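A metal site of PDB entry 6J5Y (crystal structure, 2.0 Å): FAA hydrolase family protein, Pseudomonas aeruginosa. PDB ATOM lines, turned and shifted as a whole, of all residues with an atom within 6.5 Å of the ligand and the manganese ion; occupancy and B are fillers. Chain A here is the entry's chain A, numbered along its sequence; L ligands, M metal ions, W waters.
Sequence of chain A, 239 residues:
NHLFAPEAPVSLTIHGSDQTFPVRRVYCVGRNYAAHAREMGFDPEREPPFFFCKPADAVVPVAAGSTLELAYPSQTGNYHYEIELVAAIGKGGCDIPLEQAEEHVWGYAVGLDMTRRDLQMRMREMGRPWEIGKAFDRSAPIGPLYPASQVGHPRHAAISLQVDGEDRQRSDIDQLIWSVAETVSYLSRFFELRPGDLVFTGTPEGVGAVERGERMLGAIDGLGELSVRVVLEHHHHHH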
ATOM      1  N   CYS A  28       4.533  -4.809  -6.355  1.00  0.00           N
ATOM      2  CA  CYS A  28       5.256  -3.536  -6.260  1.00  0.00           C
ATOM      3  C   CYS A  28       4.407  -2.496  -6.987  1.00  0.00           C
ATOM      4  O   CYS A  28       3.800  -2.848  -8.045  1.00  0.00           O
ATOM      5  CB  CYS A  28       6.656  -3.617  -6.862  1.00  0.00           C
ATOM      6  SG  CYS A  28       7.724  -4.885  -6.127  1.00  0.00           S
ATOM      7  N   VAL A  29       4.312  -1.301  -6.402  1.00  0.00           N
ATOM      8  CA  VAL A  29       3.611  -0.162  -7.060  1.00  0.00           C
ATOM      9  C   VAL A  29       4.687   0.755  -7.644  1.00  0.00           C
ATOM     10  O   VAL A  29       5.622   1.163  -6.890  1.00  0.00           O
ATOM     11  CB  VAL A  29       2.667   0.594  -6.110  1.00  0.00           C
ATOM     12  CG1 VAL A  29       1.835   1.587  -6.900  1.00  0.00           C
ATOM     13  CG2 VAL A  29       1.762  -0.331  -5.310  1.00  0.00           C
ATOM     14  N   GLY A  30       4.566   1.072  -8.928  1.00  0.00           N
ATOM     15  CA  GLY A  30       5.466   1.999  -9.626  1.00  0.00           C
ATOM     16  C   GLY A  30       4.857   3.387  -9.735  1.00  0.00           C
ATOM     17  O   GLY A  30       3.613   3.497  -9.946  1.00  0.00           O
ATOM     18  N   ARG A  31       5.697   4.400  -9.578  1.00  0.00           N
ATOM     19  CA  ARG A  31       5.365   5.852  -9.711  1.00  0.00           C
ATOM     20  C   ARG A  31       4.237   6.196  -8.734  1.00  0.00           C
ATOM     21  O   ARG A  31       3.186   6.729  -9.187  1.00  0.00           O
ATOM     22  CB  ARG A  31       4.996   6.181 -11.164  1.00  0.00           C
ATOM     23  CG  ARG A  31       6.181   6.160 -12.114  1.00  0.00           C
ATOM     24  CD  ARG A  31       5.830   6.421 -13.566  1.00  0.00           C
ATOM     25  NE  ARG A  31       6.774   5.725 -14.412  1.00  0.00           N
ATOM     26  CZ  ARG A  31       6.524   5.272 -15.635  1.00  0.00           C
ATOM     27  NH1 ARG A  31       5.340   5.440 -16.186  1.00  0.00           N
ATOM     28  NH2 ARG A  31       7.473   4.626 -16.303  1.00  0.00           N
ATOM     29  N   ASN A  32       4.414   5.900  -7.442  1.00  0.00           N
ATOM     30  CA  ASN A  32       3.348   6.144  -6.440  1.00  0.00           C
ATOM     31  C   ASN A  32       3.654   7.363  -5.567  1.00  0.00           C
ATOM     32  O   ASN A  32       2.942   7.537  -4.583  1.00  0.00           O
ATOM     33  CB  ASN A  32       3.099   4.931  -5.528  1.00  0.00           C
ATOM     34  CG  ASN A  32       1.671   4.841  -5.057  1.00  0.00           C
ATOM     35  OD1 ASN A  32       0.801   5.530  -5.584  1.00  0.00           O
ATOM     36  ND2 ASN A  32       1.418   3.965  -4.104  1.00  0.00           N
ATOM     37  N   TYR A  33       4.647   8.169  -5.920  1.00  0.00           N
ATOM     38  CA  TYR A  33       4.935   9.466  -5.267  1.00  0.00           C
ATOM     39  C   TYR A  33       5.070  10.475  -6.397  1.00  0.00           C
ATOM     40  O   TYR A  33       5.888  10.213  -7.286  1.00  0.00           O
ATOM     41  CB  TYR A  33       6.193   9.398  -4.403  1.00  0.00           C
ATOM     42  CG  TYR A  33       6.104   8.594  -3.123  1.00  0.00           C
ATOM     43  CD1 TYR A  33       6.227   7.223  -3.133  1.00  0.00           C
ATOM     44  CD2 TYR A  33       5.935   9.216  -1.895  1.00  0.00           C
ATOM     45  CE1 TYR A  33       6.191   6.482  -1.961  1.00  0.00           C
ATOM     46  CE2 TYR A  33       5.892   8.488  -0.710  1.00  0.00           C
ATOM     47  CZ  TYR A  33       6.016   7.101  -0.749  1.00  0.00           C
ATOM     48  OH  TYR A  33       5.959   6.347   0.395  1.00  0.00           O
ATOM     49  N   HIS A  36       8.584  11.684  -7.278  1.00  0.00           N
ATOM     50  CA  HIS A  36       9.362  10.620  -7.967  1.00  0.00           C
ATOM     51  C   HIS A  36       8.923  10.470  -9.435  1.00  0.00           C
ATOM     52  O   HIS A  36       9.808  10.380 -10.308  1.00  0.00           O
ATOM     53  CB  HIS A  36       9.231   9.273  -7.251  1.00  0.00           C
ATOM     54  CG  HIS A  36      10.029   8.193  -7.915  1.00  0.00           C
ATOM     55  ND1 HIS A  36      11.376   8.326  -8.157  1.00  0.00           N
ATOM     56  CD2 HIS A  36       9.673   6.992  -8.398  1.00  0.00           C
ATOM     57  CE1 HIS A  36      11.813   7.234  -8.771  1.00  0.00           C
ATOM     58  NE2 HIS A  36      10.792   6.401  -8.914  1.00  0.00           N
ATOM     59  N   MET A  40      11.358  11.190 -12.856  1.00  0.00           N
ATOM     60  CA  MET A  40      11.559  10.128 -13.875  1.00  0.00           C
ATOM     61  C   MET A  40      11.014  10.589 -15.235  1.00  0.00           C
ATOM     62  O   MET A  40      11.161   9.823 -16.184  1.00  0.00           O
ATOM     63  CB  MET A  40      10.902   8.820 -13.439  1.00  0.00           C
ATOM     64  CG  MET A  40      11.500   8.299 -12.141  1.00  0.00           C
ATOM     65  SD  MET A  40      13.263   7.833 -12.298  1.00  0.00           S
ATOM     66  CE  MET A  40      14.015   8.684 -10.909  1.00  0.00           C
ATOM     67  N   PHE A  50       1.086   1.937 -11.241  1.00  0.00           N
ATOM     68  CA  PHE A  50       1.031   0.633 -11.962  1.00  0.00           C
ATOM     69  C   PHE A  50       1.674  -0.450 -11.090  1.00  0.00           C
ATOM     70  O   PHE A  50       2.344  -0.177 -10.071  1.00  0.00           O
ATOM     71  CB  PHE A  50       1.712   0.734 -13.321  1.00  0.00           C
ATOM     72  CG  PHE A  50       3.161   1.135 -13.280  1.00  0.00           C
ATOM     73  CD1 PHE A  50       4.133   0.205 -12.942  1.00  0.00           C
ATOM     74  CD2 PHE A  50       3.557   2.430 -13.556  1.00  0.00           C
ATOM     75  CE1 PHE A  50       5.470   0.554 -12.908  1.00  0.00           C
ATOM     76  CE2 PHE A  50       4.889   2.801 -13.486  1.00  0.00           C
ATOM     77  CZ  PHE A  50       5.844   1.851 -13.182  1.00  0.00           C
ATOM     78  N   PHE A  52       3.841  -4.232 -10.696  1.00  0.00           N
ATOM     79  CA  PHE A  52       4.746  -5.301 -11.166  1.00  0.00           C
ATOM     80  C   PHE A  52       5.028  -6.215  -9.975  1.00  0.00           C
ATOM     81  O   PHE A  52       4.461  -5.971  -8.880  1.00  0.00           O
ATOM     82  CB  PHE A  52       6.006  -4.717 -11.790  1.00  0.00           C
ATOM     83  CG  PHE A  52       6.873  -3.885 -10.876  1.00  0.00           C
ATOM     84  CD1 PHE A  52       6.619  -2.529 -10.710  1.00  0.00           C
ATOM     85  CD2 PHE A  52       7.982  -4.436 -10.257  1.00  0.00           C
ATOM     86  CE1 PHE A  52       7.448  -1.739  -9.938  1.00  0.00           C
ATOM     87  CE2 PHE A  52       8.792  -3.650  -9.446  1.00  0.00           C
ATOM     88  CZ  PHE A  52       8.506  -2.302  -9.273  1.00  0.00           C
ATOM     89  N   GLU A  82      15.854   2.016  -3.928  1.00  0.00           N
ATOM     90  CA  GLU A  82      14.520   2.658  -3.798  1.00  0.00           C
ATOM     91  C   GLU A  82      13.923   2.280  -2.436  1.00  0.00           C
ATOM     92  O   GLU A  82      13.526   1.090  -2.310  1.00  0.00           O
ATOM     93  CB  GLU A  82      13.548   2.123  -4.864  1.00  0.00           C
ATOM     94  CG  GLU A  82      13.924   2.405  -6.305  1.00  0.00           C
ATOM     95  CD  GLU A  82      12.831   2.067  -7.313  1.00  0.00           C
ATOM     96  OE1 GLU A  82      11.800   1.538  -6.893  1.00  0.00           O
ATOM     97  OE2 GLU A  82      13.025   2.286  -8.517  1.00  0.00           O
ATOM     98  N   ILE A  83      13.831   3.215  -1.460  1.00  0.00           N
ATOM     99  CA  ILE A  83      13.236   2.895  -0.125  1.00  0.00           C
ATOM    100  C   ILE A  83      11.711   2.844  -0.279  1.00  0.00           C
ATOM    101  O   ILE A  83      11.166   3.663  -1.050  1.00  0.00           O
ATOM    102  CB  ILE A  83      13.710   3.871   0.969  1.00  0.00           C
ATOM    103  CG1 ILE A  83      13.504   3.310   2.368  1.00  0.00           C
ATOM    104  CG2 ILE A  83      13.064   5.234   0.821  1.00  0.00           C
ATOM    105  CD1 ILE A  83      14.279   2.034   2.630  1.00  0.00           C
ATOM    106  N   GLU A  84      11.030   1.909   0.407  1.00  0.00           N
ATOM    107  CA  GLU A  84       9.567   1.728   0.232  1.00  0.00           C
ATOM    108  C   GLU A  84       8.963   1.193   1.536  1.00  0.00           C
ATOM    109  O   GLU A  84       9.612   0.332   2.192  1.00  0.00           O
ATOM    110  CB  GLU A  84       9.263   0.780  -0.935  1.00  0.00           C
ATOM    111  CG  GLU A  84      10.010   1.082  -2.219  1.00  0.00           C
ATOM    112  CD  GLU A  84       9.332   0.662  -3.515  1.00  0.00           C
ATOM    113  OE1 GLU A  84       8.201   0.076  -3.479  1.00  0.00           O
ATOM    114  OE2 GLU A  84       9.921   0.951  -4.584  1.00  0.00           O
ATOM    115  N   ASP A 113      13.413  -1.655  -3.093  1.00  0.00           N
ATOM    116  CA  ASP A 113      13.116  -2.175  -4.439  1.00  0.00           C
ATOM    117  C   ASP A 113      14.390  -1.972  -5.264  1.00  0.00           C
ATOM    118  O   ASP A 113      14.454  -0.988  -6.047  1.00  0.00           O
ATOM    119  CB  ASP A 113      11.841  -1.519  -4.978  1.00  0.00           C
ATOM    120  CG  ASP A 113      11.554  -1.906  -6.418  1.00  0.00           C
ATOM    121  OD1 ASP A 113      12.172  -2.897  -6.889  1.00  0.00           O
ATOM    122  OD2 ASP A 113      10.742  -1.205  -7.062  1.00  0.00           O
ATOM    123  N   THR A 115      17.093  -2.215  -8.140  1.00  0.00           N
ATOM    124  CA  THR A 115      16.662  -2.054  -9.550  1.00  0.00           C
ATOM    125  C   THR A 115      17.884  -2.050 -10.461  1.00  0.00           C
ATOM    126  O   THR A 115      18.790  -1.295 -10.167  1.00  0.00           O
ATOM    127  CB  THR A 115      15.838  -0.767  -9.714  1.00  0.00           C
ATOM    128  OG1 THR A 115      14.669  -0.877  -8.896  1.00  0.00           O
ATOM    129  CG2 THR A 115      15.421  -0.516 -11.146  1.00  0.00           C
ATOM    130  N   ARG A 117      18.573  -0.380 -13.206  1.00  0.00           N
ATOM    131  CA  ARG A 117      17.855   0.769 -13.853  1.00  0.00           C
ATOM    132  C   ARG A 117      18.088   0.793 -15.383  1.00  0.00           C
ATOM    133  O   ARG A 117      17.103   1.074 -16.122  1.00  0.00           O
ATOM    134  CB  ARG A 117      18.262   2.090 -13.192  1.00  0.00           C
ATOM    135  CG  ARG A 117      17.559   3.326 -13.737  1.00  0.00           C
ATOM    136  CD  ARG A 117      16.101   3.417 -13.339  1.00  0.00           C
ATOM    137  NE  ARG A 117      16.024   3.607 -11.893  1.00  0.00           N
ATOM    138  CZ  ARG A 117      14.971   3.344 -11.119  1.00  0.00           C
ATOM    139  NH1 ARG A 117      13.857   2.830 -11.607  1.00  0.00           N
ATOM    140  NH2 ARG A 117      15.059   3.581  -9.828  1.00  0.00           N
ATOM    141  N   GLN A 120      15.830  -1.883 -16.774  1.00  0.00           N
ATOM    142  CA  GLN A 120      14.423  -1.471 -16.619  1.00  0.00           C
ATOM    143  C   GLN A 120      14.078  -0.410 -17.674  1.00  0.00           C
ATOM    144  O   GLN A 120      12.984  -0.476 -18.293  1.00  0.00           O
ATOM    145  CB  GLN A 120      14.182  -0.973 -15.187  1.00  0.00           C
ATOM    146  CG  GLN A 120      12.768  -0.437 -14.964  1.00  0.00           C
ATOM    147  CD  GLN A 120      12.716   1.060 -15.071  1.00  0.00           C
ATOM    148  OE1 GLN A 120      13.576   1.772 -14.550  1.00  0.00           O
ATOM    149  NE2 GLN A 120      11.710   1.577 -15.769  1.00  0.00           N
ATOM    150  N   TRP A 130       9.374  -5.882 -17.658  1.00  0.00           N
ATOM    151  CA  TRP A 130      10.464  -5.250 -16.865  1.00  0.00           C
ATOM    152  C   TRP A 130      11.248  -6.261 -16.037  1.00  0.00           C
ATOM    153  O   TRP A 130      12.138  -5.807 -15.321  1.00  0.00           O
ATOM    154  CB  TRP A 130       9.853  -4.203 -15.939  1.00  0.00           C
ATOM    155  CG  TRP A 130       9.405  -2.954 -16.618  1.00  0.00           C
ATOM    156  CD1 TRP A 130       9.089  -2.761 -17.925  1.00  0.00           C
ATOM    157  CD2 TRP A 130       9.137  -1.721 -15.936  1.00  0.00           C
ATOM    158  NE1 TRP A 130       8.673  -1.456 -18.121  1.00  0.00           N
ATOM    159  CE2 TRP A 130       8.675  -0.813 -16.916  1.00  0.00           C
ATOM    160  CE3 TRP A 130       9.204  -1.321 -14.607  1.00  0.00           C
ATOM    161  CZ2 TRP A 130       8.331   0.487 -16.591  1.00  0.00           C
ATOM    162  CZ3 TRP A 130       8.883  -0.023 -14.285  1.00  0.00           C
ATOM    163  CH2 TRP A 130       8.450   0.864 -15.273  1.00  0.00           C
ATOM    164  N   LYS A 134      13.680  -5.597 -12.673  1.00  0.00           N
ATOM    165  CA  LYS A 134      12.956  -5.520 -11.375  1.00  0.00           C
ATOM    166  C   LYS A 134      12.866  -6.864 -10.656  1.00  0.00           C
ATOM    167  O   LYS A 134      12.722  -6.864  -9.416  1.00  0.00           O
ATOM    168  CB  LYS A 134      11.536  -4.982 -11.590  1.00  0.00           C
ATOM    169  CG  LYS A 134      11.467  -3.486 -11.883  1.00  0.00           C
ATOM    170  CD  LYS A 134      11.958  -2.694 -10.706  1.00  0.00           C
ATOM    171  CE  LYS A 134      11.595  -1.232 -10.729  1.00  0.00           C
ATOM    172  NZ  LYS A 134      11.891  -0.634  -9.418  1.00  0.00           N
ATOM    173  N   PHE A 200       5.048  -3.727  -1.927  1.00  0.00           N
ATOM    174  CA  PHE A 200       5.996  -2.597  -1.979  1.00  0.00           C
ATOM    175  C   PHE A 200       5.217  -1.418  -2.582  1.00  0.00           C
ATOM    176  O   PHE A 200       4.787  -1.514  -3.724  1.00  0.00           O
ATOM    177  CB  PHE A 200       7.235  -3.002  -2.779  1.00  0.00           C
ATOM    178  CG  PHE A 200       8.246  -3.847  -2.056  1.00  0.00           C
ATOM    179  CD1 PHE A 200       7.903  -5.108  -1.563  1.00  0.00           C
ATOM    180  CD2 PHE A 200       9.560  -3.413  -1.894  1.00  0.00           C
ATOM    181  CE1 PHE A 200       8.838  -5.887  -0.900  1.00  0.00           C
ATOM    182  CE2 PHE A 200      10.492  -4.214  -1.239  1.00  0.00           C
ATOM    183  CZ  PHE A 200      10.142  -5.441  -0.754  1.00  0.00           C
ATOM    184  N   THR A 201       4.985  -0.364  -1.810  1.00  0.00           N
ATOM    185  CA  THR A 201       4.021   0.700  -2.156  1.00  0.00           C
ATOM    186  C   THR A 201       4.647   1.792  -3.039  1.00  0.00           C
ATOM    187  O   THR A 201       3.908   2.753  -3.363  1.00  0.00           O
ATOM    188  CB  THR A 201       3.441   1.296  -0.876  1.00  0.00           C
ATOM    189  OG1 THR A 201       4.514   1.763  -0.050  1.00  0.00           O
ATOM    190  CG2 THR A 201       2.610   0.271  -0.135  1.00  0.00           C
ATOM    191  N   GLY A 202       5.927   1.678  -3.387  1.00  0.00           N
ATOM    192  CA  GLY A 202       6.599   2.628  -4.300  1.00  0.00           C
ATOM    193  C   GLY A 202       7.606   3.500  -3.562  1.00  0.00           C
ATOM    194  O   GLY A 202       7.613   3.518  -2.307  1.00  0.00           O
ATOM    195  N   THR A 203       8.408   4.247  -4.313  1.00  0.00           N
ATOM    196  CA  THR A 203       9.545   5.003  -3.752  1.00  0.00           C
ATOM    197  C   THR A 203       9.383   6.512  -3.987  1.00  0.00           C
ATOM    198  O   THR A 203       8.962   6.953  -5.055  1.00  0.00           O
ATOM    199  CB  THR A 203      10.863   4.449  -4.290  1.00  0.00           C
ATOM    200  OG1 THR A 203      11.885   4.876  -3.391  1.00  0.00           O
ATOM    201  CG2 THR A 203      11.144   4.845  -5.728  1.00  0.00           C
ATOM    202  N   PRO A 204       9.727   7.328  -2.968  1.00  0.00           N
ATOM    203  CA  PRO A 204       9.709   8.774  -3.112  1.00  0.00           C
ATOM    204  C   PRO A 204      10.867   9.207  -4.015  1.00  0.00           C
ATOM    205  O   PRO A 204      11.586   8.359  -4.529  1.00  0.00           O
ATOM    206  CB  PRO A 204       9.808   9.303  -1.669  1.00  0.00           C
ATOM    207  CG  PRO A 204      10.438   8.178  -0.868  1.00  0.00           C
ATOM    208  CD  PRO A 204      10.196   6.897  -1.633  1.00  0.00           C
HETATM  209  C1  LIG L   1       8.743   2.903  -8.166  1.00  0.00           C
HETATM  210  O1  LIG L   1       8.867   2.548  -6.978  1.00  0.00           O
HETATM  211  O2  LIG L   1       8.281   4.025  -8.490  1.00  0.00           O
HETATM  212  C2  LIG L   1       9.061   2.014  -9.071  1.00  0.00           C
HETATM  213  O3  LIG L   1       9.412   0.887  -8.680  1.00  0.00           O
HETATM  214  C3  LIG L   1       9.010   2.228 -10.560  1.00  0.00           C
HETATM  215 MN    MN M   1       9.833   0.698  -6.531  1.00  0.00          MN
HETATM  216  O   HOH W   1       6.966   5.794  -6.679  1.00  0.00           O
HETATM  217  O   HOH W   2       7.938  -0.308  -6.238  1.00  0.00           O
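N of Thr 203 lies close to O1 of the ligand (3.2 Å). The backbone NH (N) of Arg 31 sits at hydrogen-bond distance from an oxygen (O2) of the ligand, at 2.8 Å. A ring nitrogen (NE2) of His 36 sits close to an oxygen (O2) of the ligand. The side-chain amino group of Lys 134 lies close to an oxygen (O3) of the ligand, 3.0 Å away.
The side-chain hydroxyl (OG1) of Thr 115 lies within hydrogen-bond range of the backbone carbonyl oxygen (O) of Asp 113, 2.9 Å away. The side-chain carboxylate (OE2) of Glu 82 is in salt-bridge range of the guanidinium group (NH2) of Arg 117, at 2.7 Å. The side-chain hydroxyl (OG1) of Thr 115 is in hydrogen-bond range of the side-chain amino group (NZ) of Lys 134 (2.8 Å). N of Gly 30 is in hydrogen-bond range of O of Phe 50, at 2.8 Å. N of Val 29 is in hydrogen-bond range of O of Phe 200, 2.7 Å away. OE1 of Glu 84 sits at hydrogen-bond distance from N of Gly 202, at 2.8 Å. The backbone carbonyl oxygen (O) of Phe 52 lies within hydrogen-bond range of the backbone NH (N) of Cys 28 (2.8 Å). The side-chain carboxylate (OD1) of Asp 113 is in salt-bridge range of the side-chain amino group (NZ) of Lys 134 (3.4 Å).
Val 29 touches the ligand (O to O1, 3.5 Å). CA of Gly 30 touches C2 of the ligand, 3.6 Å away. Phe 52 touches the ligand (CZ to O3, 3.4 Å). Gly 202 touches the ligand (CA to O1, 3.5 Å). Hydrophobic or aromatic side chains that line the ligand: His 36 and Phe 52.
Merely in contact with the manganese ion: Lys 134 (3.8 Å). Four residues have an atom within 4 Å of the manganese ion: Glu 82, Glu 84, Asp 113 and Lys 134. The nearest printed residue that does not touch the manganese ion is Val 29 (4.3 Å).
The manganese ion is bound by OE2 of Glu 84, at 2.0 Å. The manganese ion is bound by O1 of the ligand (2.1 Å). Water W2 is bound to the manganese ion, at 2.2 Å. OE1 of Glu 82 binds the manganese ion (2.2 Å). The side-chain carboxylate (OD2) of Asp 113 binds the manganese ion (2.2 Å). The manganese ion is bound by O3 of the ligand, 2.2 Å away.
Water W2 bridges OE1 of Glu 84 (2.8 Å) and O of Val 29 (2.8 Å).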
